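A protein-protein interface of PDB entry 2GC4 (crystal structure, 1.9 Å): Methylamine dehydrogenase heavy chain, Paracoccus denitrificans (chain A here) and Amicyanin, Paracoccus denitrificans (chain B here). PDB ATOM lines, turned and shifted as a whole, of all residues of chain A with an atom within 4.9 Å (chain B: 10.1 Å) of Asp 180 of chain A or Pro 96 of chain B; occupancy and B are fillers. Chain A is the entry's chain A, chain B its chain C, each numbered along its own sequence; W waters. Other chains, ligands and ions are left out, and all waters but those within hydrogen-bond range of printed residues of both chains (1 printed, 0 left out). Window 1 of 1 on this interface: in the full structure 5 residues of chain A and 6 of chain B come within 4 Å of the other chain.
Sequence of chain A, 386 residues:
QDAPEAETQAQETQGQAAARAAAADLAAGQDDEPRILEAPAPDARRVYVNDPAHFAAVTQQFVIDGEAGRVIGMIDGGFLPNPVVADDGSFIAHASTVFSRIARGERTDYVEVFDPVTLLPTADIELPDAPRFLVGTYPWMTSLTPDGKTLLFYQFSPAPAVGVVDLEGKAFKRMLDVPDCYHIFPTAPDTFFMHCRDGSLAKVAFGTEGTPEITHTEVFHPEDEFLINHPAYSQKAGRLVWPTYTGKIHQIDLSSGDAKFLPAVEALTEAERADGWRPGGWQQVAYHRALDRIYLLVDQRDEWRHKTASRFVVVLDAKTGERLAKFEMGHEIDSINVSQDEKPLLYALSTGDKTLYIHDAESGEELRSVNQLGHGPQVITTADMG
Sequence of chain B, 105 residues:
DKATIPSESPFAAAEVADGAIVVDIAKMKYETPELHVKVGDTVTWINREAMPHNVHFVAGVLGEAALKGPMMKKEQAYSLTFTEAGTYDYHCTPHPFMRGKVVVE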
ATOM      1  N   PHE A 156       9.680  -6.974   7.214  1.00  0.00           N
ATOM      2  CA  PHE A 156      10.339  -7.023   8.517  1.00  0.00           C
ATOM      3  C   PHE A 156      11.853  -7.011   8.396  1.00  0.00           C
ATOM      4  O   PHE A 156      12.535  -6.209   9.035  1.00  0.00           O
ATOM      5  CB  PHE A 156       9.903  -8.292   9.259  1.00  0.00           C
ATOM      6  CG  PHE A 156      10.546  -8.474  10.604  1.00  0.00           C
ATOM      7  CD1 PHE A 156      10.194  -7.664  11.678  1.00  0.00           C
ATOM      8  CD2 PHE A 156      11.489  -9.480  10.806  1.00  0.00           C
ATOM      9  CE1 PHE A 156      10.771  -7.853  12.939  1.00  0.00           C
ATOM     10  CE2 PHE A 156      12.073  -9.677  12.063  1.00  0.00           C
ATOM     11  CZ  PHE A 156      11.715  -8.867  13.127  1.00  0.00           C
ATOM     12  N   PRO A 158      15.355  -7.310   5.601  1.00  0.00           N
ATOM     13  CA  PRO A 158      16.484  -6.967   6.477  1.00  0.00           C
ATOM     14  C   PRO A 158      16.245  -5.749   7.362  1.00  0.00           C
ATOM     15  O   PRO A 158      16.898  -5.582   8.394  1.00  0.00           O
ATOM     16  CB  PRO A 158      17.629  -6.712   5.492  1.00  0.00           C
ATOM     17  CG  PRO A 158      17.209  -7.442   4.248  1.00  0.00           C
ATOM     18  CD  PRO A 158      15.744  -7.148   4.190  1.00  0.00           C
ATOM     19  N   PRO A 160      12.982  -2.590   8.541  1.00  0.00           N
ATOM     20  CA  PRO A 160      11.574  -2.181   8.501  1.00  0.00           C
ATOM     21  C   PRO A 160      11.294  -1.368   7.237  1.00  0.00           C
ATOM     22  O   PRO A 160      11.993  -0.396   6.955  1.00  0.00           O
ATOM     23  CB  PRO A 160      11.423  -1.334   9.765  1.00  0.00           C
ATOM     24  CG  PRO A 160      12.449  -1.915  10.693  1.00  0.00           C
ATOM     25  CD  PRO A 160      13.631  -2.135   9.784  1.00  0.00           C
ATOM     26  N   VAL A 178      11.118   2.922   6.985  1.00  0.00           N
ATOM     27  CA  VAL A 178      10.439   3.446   8.157  1.00  0.00           C
ATOM     28  C   VAL A 178      11.193   3.045   9.415  1.00  0.00           C
ATOM     29  O   VAL A 178      12.067   2.181   9.368  1.00  0.00           O
ATOM     30  CB  VAL A 178       8.989   2.902   8.238  1.00  0.00           C
ATOM     31  CG1 VAL A 178       8.241   3.231   6.953  1.00  0.00           C
ATOM     32  CG2 VAL A 178       9.000   1.400   8.466  1.00  0.00           C
ATOM     33  N   PRO A 179      10.875   3.679  10.552  1.00  0.00           N
ATOM     34  CA  PRO A 179      11.545   3.356  11.814  1.00  0.00           C
ATOM     35  C   PRO A 179      11.099   1.967  12.262  1.00  0.00           C
ATOM     36  O   PRO A 179      10.372   1.274  11.538  1.00  0.00           O
ATOM     37  CB  PRO A 179      11.051   4.446  12.766  1.00  0.00           C
ATOM     38  CG  PRO A 179      10.653   5.579  11.841  1.00  0.00           C
ATOM     39  CD  PRO A 179       9.988   4.845  10.715  1.00  0.00           C
ATOM     40  N   ASP A 180      11.527   1.568  13.454  1.00  0.00           N
ATOM     41  CA  ASP A 180      11.166   0.270  14.001  1.00  0.00           C
ATOM     42  C   ASP A 180       9.718   0.324  14.485  1.00  0.00           C
ATOM     43  O   ASP A 180       9.446   0.430  15.683  1.00  0.00           O
ATOM     44  CB  ASP A 180      12.111  -0.082  15.148  1.00  0.00           C
ATOM     45  CG  ASP A 180      13.558  -0.188  14.690  1.00  0.00           C
ATOM     46  OD1 ASP A 180      13.851  -1.082  13.864  1.00  0.00           O
ATOM     47  OD2 ASP A 180      14.399   0.620  15.145  1.00  0.00           O
ATOM     48  N   CYS A 181       8.798   0.260  13.530  1.00  0.00           N
ATOM     49  CA  CYS A 181       7.373   0.310  13.812  1.00  0.00           C
ATOM     50  C   CYS A 181       6.683  -0.810  13.035  1.00  0.00           C
ATOM     51  O   CYS A 181       7.251  -1.355  12.083  1.00  0.00           O
ATOM     52  CB  CYS A 181       6.824   1.679  13.413  1.00  0.00           C
ATOM     53  SG  CYS A 181       7.844   3.046  14.065  1.00  0.00           S
ATOM     54  N   TYR A 182       5.456  -1.135  13.442  1.00  0.00           N
ATOM     55  CA  TYR A 182       4.705  -2.232  12.850  1.00  0.00           C
ATOM     56  C   TYR A 182       3.238  -1.902  12.581  1.00  0.00           C
ATOM     57  O   TYR A 182       2.665  -1.038  13.233  1.00  0.00           O
ATOM     58  CB  TYR A 182       4.799  -3.442  13.782  1.00  0.00           C
ATOM     59  CG  TYR A 182       6.216  -3.709  14.248  1.00  0.00           C
ATOM     60  CD1 TYR A 182       6.838  -2.870  15.178  1.00  0.00           C
ATOM     61  CD2 TYR A 182       6.960  -4.747  13.701  1.00  0.00           C
ATOM     62  CE1 TYR A 182       8.172  -3.059  15.543  1.00  0.00           C
ATOM     63  CE2 TYR A 182       8.292  -4.946  14.059  1.00  0.00           C
ATOM     64  CZ  TYR A 182       8.891  -4.099  14.977  1.00  0.00           C
ATOM     65  OH  TYR A 182      10.212  -4.295  15.321  1.00  0.00           O
ATOM     66  N   HIS A 195       2.629   1.559  14.464  1.00  0.00           N
ATOM     67  CA  HIS A 195       2.840   1.522  15.906  1.00  0.00           C
ATOM     68  C   HIS A 195       4.300   1.139  16.112  1.00  0.00           C
ATOM     69  O   HIS A 195       4.769   0.146  15.549  1.00  0.00           O
ATOM     70  CB  HIS A 195       1.938   0.488  16.577  1.00  0.00           C
ATOM     71  CG  HIS A 195       2.282   0.245  18.014  1.00  0.00           C
ATOM     72  ND1 HIS A 195       2.686  -0.986  18.485  1.00  0.00           N
ATOM     73  CD2 HIS A 195       2.308   1.083  19.077  1.00  0.00           C
ATOM     74  CE1 HIS A 195       2.947  -0.895  19.777  1.00  0.00           C
ATOM     75  NE2 HIS A 195       2.725   0.351  20.159  1.00  0.00           N
ATOM     76  N   CYS A 196       5.008   1.913  16.931  1.00  0.00           N
ATOM     77  CA  CYS A 196       6.430   1.675  17.159  1.00  0.00           C
ATOM     78  C   CYS A 196       6.817   1.000  18.476  1.00  0.00           C
ATOM     79  O   CYS A 196       6.081   1.047  19.468  1.00  0.00           O
ATOM     80  CB  CYS A 196       7.176   2.998  17.020  1.00  0.00           C
ATOM     81  SG  CYS A 196       6.715   3.911  15.511  1.00  0.00           S
ATOM     82  N   ARG A 197       7.993   0.378  18.463  1.00  0.00           N
ATOM     83  CA  ARG A 197       8.535  -0.323  19.626  1.00  0.00           C
ATOM     84  C   ARG A 197       8.619   0.572  20.866  1.00  0.00           C
ATOM     85  O   ARG A 197       8.443   0.095  21.983  1.00  0.00           O
ATOM     86  CB  ARG A 197       9.929  -0.870  19.296  1.00  0.00           C
ATOM     87  CG  ARG A 197      10.549  -1.747  20.398  1.00  0.00           C
ATOM     88  CD  ARG A 197      11.996  -2.104  20.065  1.00  0.00           C
ATOM     89  NE  ARG A 197      12.672  -2.809  21.156  1.00  0.00           N
ATOM     90  CZ  ARG A 197      12.599  -4.119  21.373  1.00  0.00           C
ATOM     91  NH1 ARG A 197      13.251  -4.659  22.395  1.00  0.00           N
ATOM     92  NH2 ARG A 197      11.890  -4.896  20.565  1.00  0.00           N
ATOM     93  N   MET B  28      20.521  -6.392  24.708  1.00  0.00           N
ATOM     94  CA  MET B  28      19.942  -6.072  23.406  1.00  0.00           C
ATOM     95  C   MET B  28      20.616  -4.925  22.670  1.00  0.00           C
ATOM     96  O   MET B  28      19.947  -4.154  21.980  1.00  0.00           O
ATOM     97  CB  MET B  28      18.451  -5.748  23.559  1.00  0.00           C
ATOM     98  CG  MET B  28      17.634  -6.847  24.205  1.00  0.00           C
ATOM     99  SD  MET B  28      17.699  -8.381  23.274  1.00  0.00           S
ATOM    100  CE  MET B  28      16.499  -8.051  22.002  1.00  0.00           C
ATOM    101  N   TYR B  30      24.648  -3.333  20.852  1.00  0.00           N
ATOM    102  CA  TYR B  30      26.070  -3.428  20.555  1.00  0.00           C
ATOM    103  C   TYR B  30      26.604  -2.307  21.444  1.00  0.00           C
ATOM    104  O   TYR B  30      26.329  -1.133  21.193  1.00  0.00           O
ATOM    105  CB  TYR B  30      26.318  -3.137  19.073  1.00  0.00           C
ATOM    106  CG  TYR B  30      25.678  -4.162  18.159  1.00  0.00           C
ATOM    107  CD1 TYR B  30      26.114  -5.489  18.153  1.00  0.00           C
ATOM    108  CD2 TYR B  30      24.621  -3.812  17.314  1.00  0.00           C
ATOM    109  CE1 TYR B  30      25.512  -6.449  17.327  1.00  0.00           C
ATOM    110  CE2 TYR B  30      24.010  -4.765  16.482  1.00  0.00           C
ATOM    111  CZ  TYR B  30      24.460  -6.076  16.494  1.00  0.00           C
ATOM    112  OH  TYR B  30      23.869  -7.011  15.669  1.00  0.00           O
ATOM    113  N   PRO B  52      20.594 -15.039  21.961  1.00  0.00           N
ATOM    114  CA  PRO B  52      21.475 -15.148  20.792  1.00  0.00           C
ATOM    115  C   PRO B  52      21.434 -13.899  19.907  1.00  0.00           C
ATOM    116  O   PRO B  52      20.380 -13.283  19.749  1.00  0.00           O
ATOM    117  CB  PRO B  52      20.938 -16.385  20.072  1.00  0.00           C
ATOM    118  CG  PRO B  52      20.382 -17.221  21.209  1.00  0.00           C
ATOM    119  CD  PRO B  52      19.656 -16.175  22.017  1.00  0.00           C
ATOM    120  N   HIS B  53      22.584 -13.539  19.337  1.00  0.00           N
ATOM    121  CA  HIS B  53      22.713 -12.365  18.462  1.00  0.00           C
ATOM    122  C   HIS B  53      23.737 -12.656  17.360  1.00  0.00           C
ATOM    123  O   HIS B  53      24.525 -13.591  17.466  1.00  0.00           O
ATOM    124  CB  HIS B  53      23.228 -11.142  19.235  1.00  0.00           C
ATOM    125  CG  HIS B  53      22.361 -10.712  20.378  1.00  0.00           C
ATOM    126  ND1 HIS B  53      21.127 -10.119  20.234  1.00  0.00           N
ATOM    127  CD2 HIS B  53      22.602 -10.734  21.712  1.00  0.00           C
ATOM    128  CE1 HIS B  53      20.674  -9.796  21.453  1.00  0.00           C
ATOM    129  NE2 HIS B  53      21.534 -10.150  22.388  1.00  0.00           N
ATOM    130  N   ASN B  54      23.735 -11.829  16.321  1.00  0.00           N
ATOM    131  CA  ASN B  54      24.672 -11.975  15.215  1.00  0.00           C
ATOM    132  C   ASN B  54      24.851 -10.592  14.598  1.00  0.00           C
ATOM    133  O   ASN B  54      24.272  -9.617  15.076  1.00  0.00           O
ATOM    134  CB  ASN B  54      24.108 -12.941  14.161  1.00  0.00           C
ATOM    135  CG  ASN B  54      23.085 -12.280  13.231  1.00  0.00           C
ATOM    136  OD1 ASN B  54      22.325 -11.400  13.636  1.00  0.00           O
ATOM    137  ND2 ASN B  54      23.056 -12.725  11.980  1.00  0.00           N
ATOM    138  N   HIS B  56      24.746  -8.536  10.834  1.00  0.00           N
ATOM    139  CA  HIS B  56      24.206  -8.712   9.498  1.00  0.00           C
ATOM    140  C   HIS B  56      24.374  -7.436   8.682  1.00  0.00           C
ATOM    141  O   HIS B  56      23.884  -6.370   9.065  1.00  0.00           O
ATOM    142  CB  HIS B  56      22.723  -9.100   9.630  1.00  0.00           C
ATOM    143  CG  HIS B  56      22.010  -9.314   8.330  1.00  0.00           C
ATOM    144  ND1 HIS B  56      20.709  -9.765   8.270  1.00  0.00           N
ATOM    145  CD2 HIS B  56      22.398  -9.109   7.047  1.00  0.00           C
ATOM    146  CE1 HIS B  56      20.324  -9.826   7.007  1.00  0.00           C
ATOM    147  NE2 HIS B  56      21.328  -9.433   6.246  1.00  0.00           N
ATOM    148  N   VAL B  58      23.626  -5.774   5.042  1.00  0.00           N
ATOM    149  CA  VAL B  58      22.803  -5.952   3.852  1.00  0.00           C
ATOM    150  C   VAL B  58      23.660  -5.983   2.589  1.00  0.00           C
ATOM    151  O   VAL B  58      24.811  -5.536   2.594  1.00  0.00           O
ATOM    152  CB  VAL B  58      21.738  -4.834   3.725  1.00  0.00           C
ATOM    153  CG1 VAL B  58      20.825  -4.850   4.944  1.00  0.00           C
ATOM    154  CG2 VAL B  58      22.407  -3.480   3.574  1.00  0.00           C
ATOM    155  N   MET B  71      24.721 -16.946  14.249  1.00  0.00           N
ATOM    156  CA  MET B  71      24.196 -16.541  15.548  1.00  0.00           C
ATOM    157  C   MET B  71      25.176 -16.953  16.644  1.00  0.00           C
ATOM    158  O   MET B  71      25.678 -18.079  16.652  1.00  0.00           O
ATOM    159  CB  MET B  71      22.832 -17.192  15.807  1.00  0.00           C
ATOM    160  CG  MET B  71      21.698 -16.649  14.948  1.00  0.00           C
ATOM    161  SD  MET B  71      21.318 -14.907  15.265  1.00  0.00           S
ATOM    162  CE  MET B  71      20.383 -15.042  16.780  1.00  0.00           C
ATOM    163  N   ASP B  89      27.460  -0.227   8.042  1.00  0.00           N
ATOM    164  CA  ASP B  89      26.349  -0.402   8.964  1.00  0.00           C
ATOM    165  C   ASP B  89      25.958  -1.867   9.029  1.00  0.00           C
ATOM    166  O   ASP B  89      26.159  -2.622   8.076  1.00  0.00           O
ATOM    167  CB  ASP B  89      25.133   0.410   8.512  1.00  0.00           C
ATOM    168  CG  ASP B  89      25.440   1.880   8.348  1.00  0.00           C
ATOM    169  OD1 ASP B  89      26.215   2.226   7.432  1.00  0.00           O
ATOM    170  OD2 ASP B  89      24.911   2.688   9.136  1.00  0.00           O
ATOM    171  N   TYR B  90      25.394  -2.266  10.159  1.00  0.00           N
ATOM    172  CA  TYR B  90      24.954  -3.638  10.337  1.00  0.00           C
ATOM    173  C   TYR B  90      23.861  -3.678  11.395  1.00  0.00           C
ATOM    174  O   TYR B  90      23.626  -2.688  12.098  1.00  0.00           O
ATOM    175  CB  TYR B  90      26.125  -4.542  10.756  1.00  0.00           C
ATOM    176  CG  TYR B  90      26.755  -4.191  12.089  1.00  0.00           C
ATOM    177  CD1 TYR B  90      27.760  -3.226  12.180  1.00  0.00           C
ATOM    178  CD2 TYR B  90      26.340  -4.822  13.263  1.00  0.00           C
ATOM    179  CE1 TYR B  90      28.341  -2.897  13.412  1.00  0.00           C
ATOM    180  CE2 TYR B  90      26.909  -4.500  14.499  1.00  0.00           C
ATOM    181  CZ  TYR B  90      27.909  -3.538  14.566  1.00  0.00           C
ATOM    182  OH  TYR B  90      28.470  -3.219  15.785  1.00  0.00           O
ATOM    183  N   HIS B  91      23.184  -4.819  11.486  1.00  0.00           N
ATOM    184  CA  HIS B  91      22.124  -5.010  12.468  1.00  0.00           C
ATOM    185  C   HIS B  91      22.080  -6.481  12.860  1.00  0.00           C
ATOM    186  O   HIS B  91      22.869  -7.291  12.375  1.00  0.00           O
ATOM    187  CB  HIS B  91      20.759  -4.586  11.901  1.00  0.00           C
ATOM    188  CG  HIS B  91      20.237  -5.495  10.828  1.00  0.00           C
ATOM    189  ND1 HIS B  91      20.754  -5.515   9.550  1.00  0.00           N
ATOM    190  CD2 HIS B  91      19.261  -6.435  10.854  1.00  0.00           C
ATOM    191  CE1 HIS B  91      20.119  -6.428   8.835  1.00  0.00           C
ATOM    192  NE2 HIS B  91      19.209  -7.002   9.603  1.00  0.00           N
ATOM    193  N   CYS B  92      21.157  -6.811  13.752  1.00  0.00           N
ATOM    194  CA  CYS B  92      20.976  -8.178  14.215  1.00  0.00           C
ATOM    195  C   CYS B  92      19.764  -8.755  13.469  1.00  0.00           C
ATOM    196  O   CYS B  92      18.656  -8.221  13.558  1.00  0.00           O
ATOM    197  CB  CYS B  92      20.729  -8.175  15.716  1.00  0.00           C
ATOM    198  SG  CYS B  92      20.697  -9.804  16.429  1.00  0.00           S
ATOM    199  N   THR B  93      19.984  -9.841  12.735  1.00  0.00           N
ATOM    200  CA  THR B  93      18.934 -10.466  11.935  1.00  0.00           C
ATOM    201  C   THR B  93      17.549 -10.556  12.584  1.00  0.00           C
ATOM    202  O   THR B  93      16.601  -9.967  12.080  1.00  0.00           O
ATOM    203  CB  THR B  93      19.385 -11.860  11.451  1.00  0.00           C
ATOM    204  OG1 THR B  93      20.558 -11.712  10.638  1.00  0.00           O
ATOM    205  CG2 THR B  93      18.284 -12.526  10.622  1.00  0.00           C
ATOM    206  N   PRO B  94      17.411 -11.281  13.710  1.00  0.00           N
ATOM    207  CA  PRO B  94      16.093 -11.386  14.353  1.00  0.00           C
ATOM    208  C   PRO B  94      15.646 -10.133  15.111  1.00  0.00           C
ATOM    209  O   PRO B  94      14.478 -10.014  15.495  1.00  0.00           O
ATOM    210  CB  PRO B  94      16.264 -12.583  15.289  1.00  0.00           C
ATOM    211  CG  PRO B  94      17.698 -12.458  15.704  1.00  0.00           C
ATOM    212  CD  PRO B  94      18.400 -12.134  14.399  1.00  0.00           C
ATOM    213  N   HIS B  95      16.574  -9.203  15.319  1.00  0.00           N
ATOM    214  CA  HIS B  95      16.289  -7.978  16.061  1.00  0.00           C
ATOM    215  C   HIS B  95      16.701  -6.747  15.248  1.00  0.00           C
ATOM    216  O   HIS B  95      17.683  -6.079  15.574  1.00  0.00           O
ATOM    217  CB  HIS B  95      17.060  -8.013  17.386  1.00  0.00           C
ATOM    218  CG  HIS B  95      16.947  -9.319  18.115  1.00  0.00           C
ATOM    219  ND1 HIS B  95      17.947  -9.863  18.889  1.00  0.00           N
ATOM    220  CD2 HIS B  95      15.917 -10.202  18.178  1.00  0.00           C
ATOM    221  CE1 HIS B  95      17.509 -11.032  19.381  1.00  0.00           C
ATOM    222  NE2 HIS B  95      16.278 -11.282  18.978  1.00  0.00           N
ATOM    223  N   PRO B  96      15.941  -6.423  14.186  1.00  0.00           N
ATOM    224  CA  PRO B  96      16.213  -5.277  13.306  1.00  0.00           C
ATOM    225  C   PRO B  96      16.478  -3.952  14.022  1.00  0.00           C
ATOM    226  O   PRO B  96      17.162  -3.077  13.486  1.00  0.00           O
ATOM    227  CB  PRO B  96      14.965  -5.218  12.423  1.00  0.00           C
ATOM    228  CG  PRO B  96      14.553  -6.654  12.333  1.00  0.00           C
ATOM    229  CD  PRO B  96      14.710  -7.118  13.768  1.00  0.00           C
ATOM    230  N   PHE B  97      15.939  -3.804  15.226  1.00  0.00           N
ATOM    231  CA  PHE B  97      16.130  -2.579  15.995  1.00  0.00           C
ATOM    232  C   PHE B  97      17.546  -2.456  16.563  1.00  0.00           C
ATOM    233  O   PHE B  97      17.952  -1.374  17.003  1.00  0.00           O
ATOM    234  CB  PHE B  97      15.118  -2.503  17.140  1.00  0.00           C
ATOM    235  CG  PHE B  97      15.080  -3.733  17.993  1.00  0.00           C
ATOM    236  CD1 PHE B  97      14.377  -4.860  17.577  1.00  0.00           C
ATOM    237  CD2 PHE B  97      15.761  -3.776  19.204  1.00  0.00           C
ATOM    238  CE1 PHE B  97      14.355  -6.014  18.359  1.00  0.00           C
ATOM    239  CE2 PHE B  97      15.747  -4.925  19.993  1.00  0.00           C
ATOM    240  CZ  PHE B  97      15.042  -6.045  19.569  1.00  0.00           C
ATOM    241  N   MET B  98      18.287  -3.562  16.573  1.00  0.00           N
ATOM    242  CA  MET B  98      19.666  -3.557  17.068  1.00  0.00           C
ATOM    243  C   MET B  98      20.569  -3.147  15.924  1.00  0.00           C
ATOM    244  O   MET B  98      20.726  -3.897  14.966  1.00  0.00           O
ATOM    245  CB  MET B  98      20.087  -4.949  17.526  1.00  0.00           C
ATOM    246  CG  MET B  98      19.707  -5.288  18.931  1.00  0.00           C
ATOM    247  SD  MET B  98      20.279  -6.933  19.354  1.00  0.00           S
ATOM    248  CE  MET B  98      22.046  -6.651  19.633  1.00  0.00           C
ATOM    249  N   ARG B  99      21.172  -1.968  16.027  1.00  0.00           N
ATOM    250  CA  ARG B  99      22.040  -1.487  14.967  1.00  0.00           C
ATOM    251  C   ARG B  99      23.407  -1.034  15.463  1.00  0.00           C
ATOM    252  O   ARG B  99      23.562  -0.560  16.594  1.00  0.00           O
ATOM    253  CB  ARG B  99      21.360  -0.341  14.208  1.00  0.00           C
ATOM    254  CG  ARG B  99      20.044  -0.737  13.546  1.00  0.00           C
ATOM    255  CD  ARG B  99      19.491   0.391  12.683  1.00  0.00           C
ATOM    256  NE  ARG B  99      18.223   0.030  12.058  1.00  0.00           N
ATOM    257  CZ  ARG B  99      17.063  -0.055  12.706  1.00  0.00           C
ATOM    258  NH1 ARG B  99      15.958  -0.398  12.050  1.00  0.00           N
ATOM    259  NH2 ARG B  99      17.004   0.218  14.006  1.00  0.00           N
ATOM    260  N   GLY B 100      24.396  -1.194  14.592  1.00  0.00           N
ATOM    261  CA  GLY B 100      25.754  -0.809  14.914  1.00  0.00           C
ATOM    262  C   GLY B 100      26.427  -0.259  13.675  1.00  0.00           C
ATOM    263  O   GLY B 100      25.869  -0.313  12.574  1.00  0.00           O
HETATM  264  O   HOH W   1      17.003  -8.784   9.479  1.00  0.00           O
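N of Val 178 of chain A is in hydrogen-bond range of O of Pro 160 of chain A, at 3.4 Å.
The backbone carbonyl oxygen (O) of Asp 180 of chain A sits at hydrogen-bond distance from the backbone NH (N) of Arg 197 of chain A, 3.1 Å away.
O of His 91 of chain B sits close to OH of Tyr 30 of chain B (3.5 Å).
N of His 56 of chain B is in hydrogen-bond range of O of His 91 of chain B.
O of Pro 96 of chain B lies close to NH1 of Arg 99 of chain B (3.3 Å).
The side-chain sulfur (SG) of Cys 181 of chain A forms a disulfide with the side-chain sulfur (SG) of Cys 196 of chain A (2.0 Å).
Of the 20 printed residues of chain B, 6 touch a printed residue of chain A.
Hydrophobic or aromatic side chains of chain B within 4 Å of the printed part of chain A: Val 58, His 91, Pro 96 and Phe 97.
Along chain A the printed residues that touch a printed residue of chain B span positions 156 to 197.
Among the printed residues, 9 pairs touch across the chains.
Among the printed residues, Asp or Glu carboxylates within 4 Å of a Lys or Arg side-chain nitrogen of the other chain: Asp 180 of chain A with Arg 99 of chain B (2.9 Å).
Asp 180 of chain A touches just these residues of chain B: Pro 96, Phe 97 and Arg 99.
Of chain A, only Phe 156 and Asp 180 come within 4 Å of Pro 96 of chain B.
No residue of chain B comes within 4 Å of Cys 196 of chain A.
Of the printed residues of chain B, Pro 160 of chain A touches Arg 99 (3.7 Å).
Of the printed residues of chain B, Phe 156 of chain A touches Pro 94 (3.8 Å) and Pro 96 (3.5 Å).
Printed residues of chain A within 4 Å of Arg 99 of chain B: Pro 160 (3.7 Å) and Asp 180 (2.9 Å).
Printed residues of chain A within 4 Å of Val 58 of chain B: Pro 158.
Of the printed residues of chain B, Arg 197 of chain A touches Phe 97 (3.5 Å).
The nearest residue of chain B that does not touch Asp 180 of chain A is Met 98 of chain B (5.8 Å).
The nearest residue of chain A that does not touch Pro 96 of chain B is Pro 160 of chain A (4.3 Å).
Water W1 lies within hydrogen-bond range of a ring nitrogen (NE2) of His 91 of chain B (2.8 Å), the backbone carbonyl oxygen (O) of Thr 93 of chain B (2.9 Å) and the backbone carbonyl oxygen (O) of Pro 158 of chain A (3.4 Å).
Among the printed residues, pairs that only touch across the chains: Phe 156 of chain A with Pro 94 of chain B (3.8 Å), Phe 156 of chain A with Pro 96 of chain B (3.5 Å), Pro 158 of chain A with Val 58 of chain B (3.7 Å), Pro 160 of chain A with Arg 99 of chain B (3.7 Å), Asp 180 of chain A with Pro 96 of chain B (3.9 Å), Asp 180 of chain A with Phe 97 of chain B (3.5 Å) and Arg 197 of chain A with Phe 97 of chain B (3.5 Å).
NE2 of His 91 of chain B sits at hydrogen-bond distance from O of Pro 158 of chain A (3.0 Å).
OD1 of Asp 180 of chain A is in salt-bridge range of NH1 of Arg 99 of chain B (2.9 Å).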
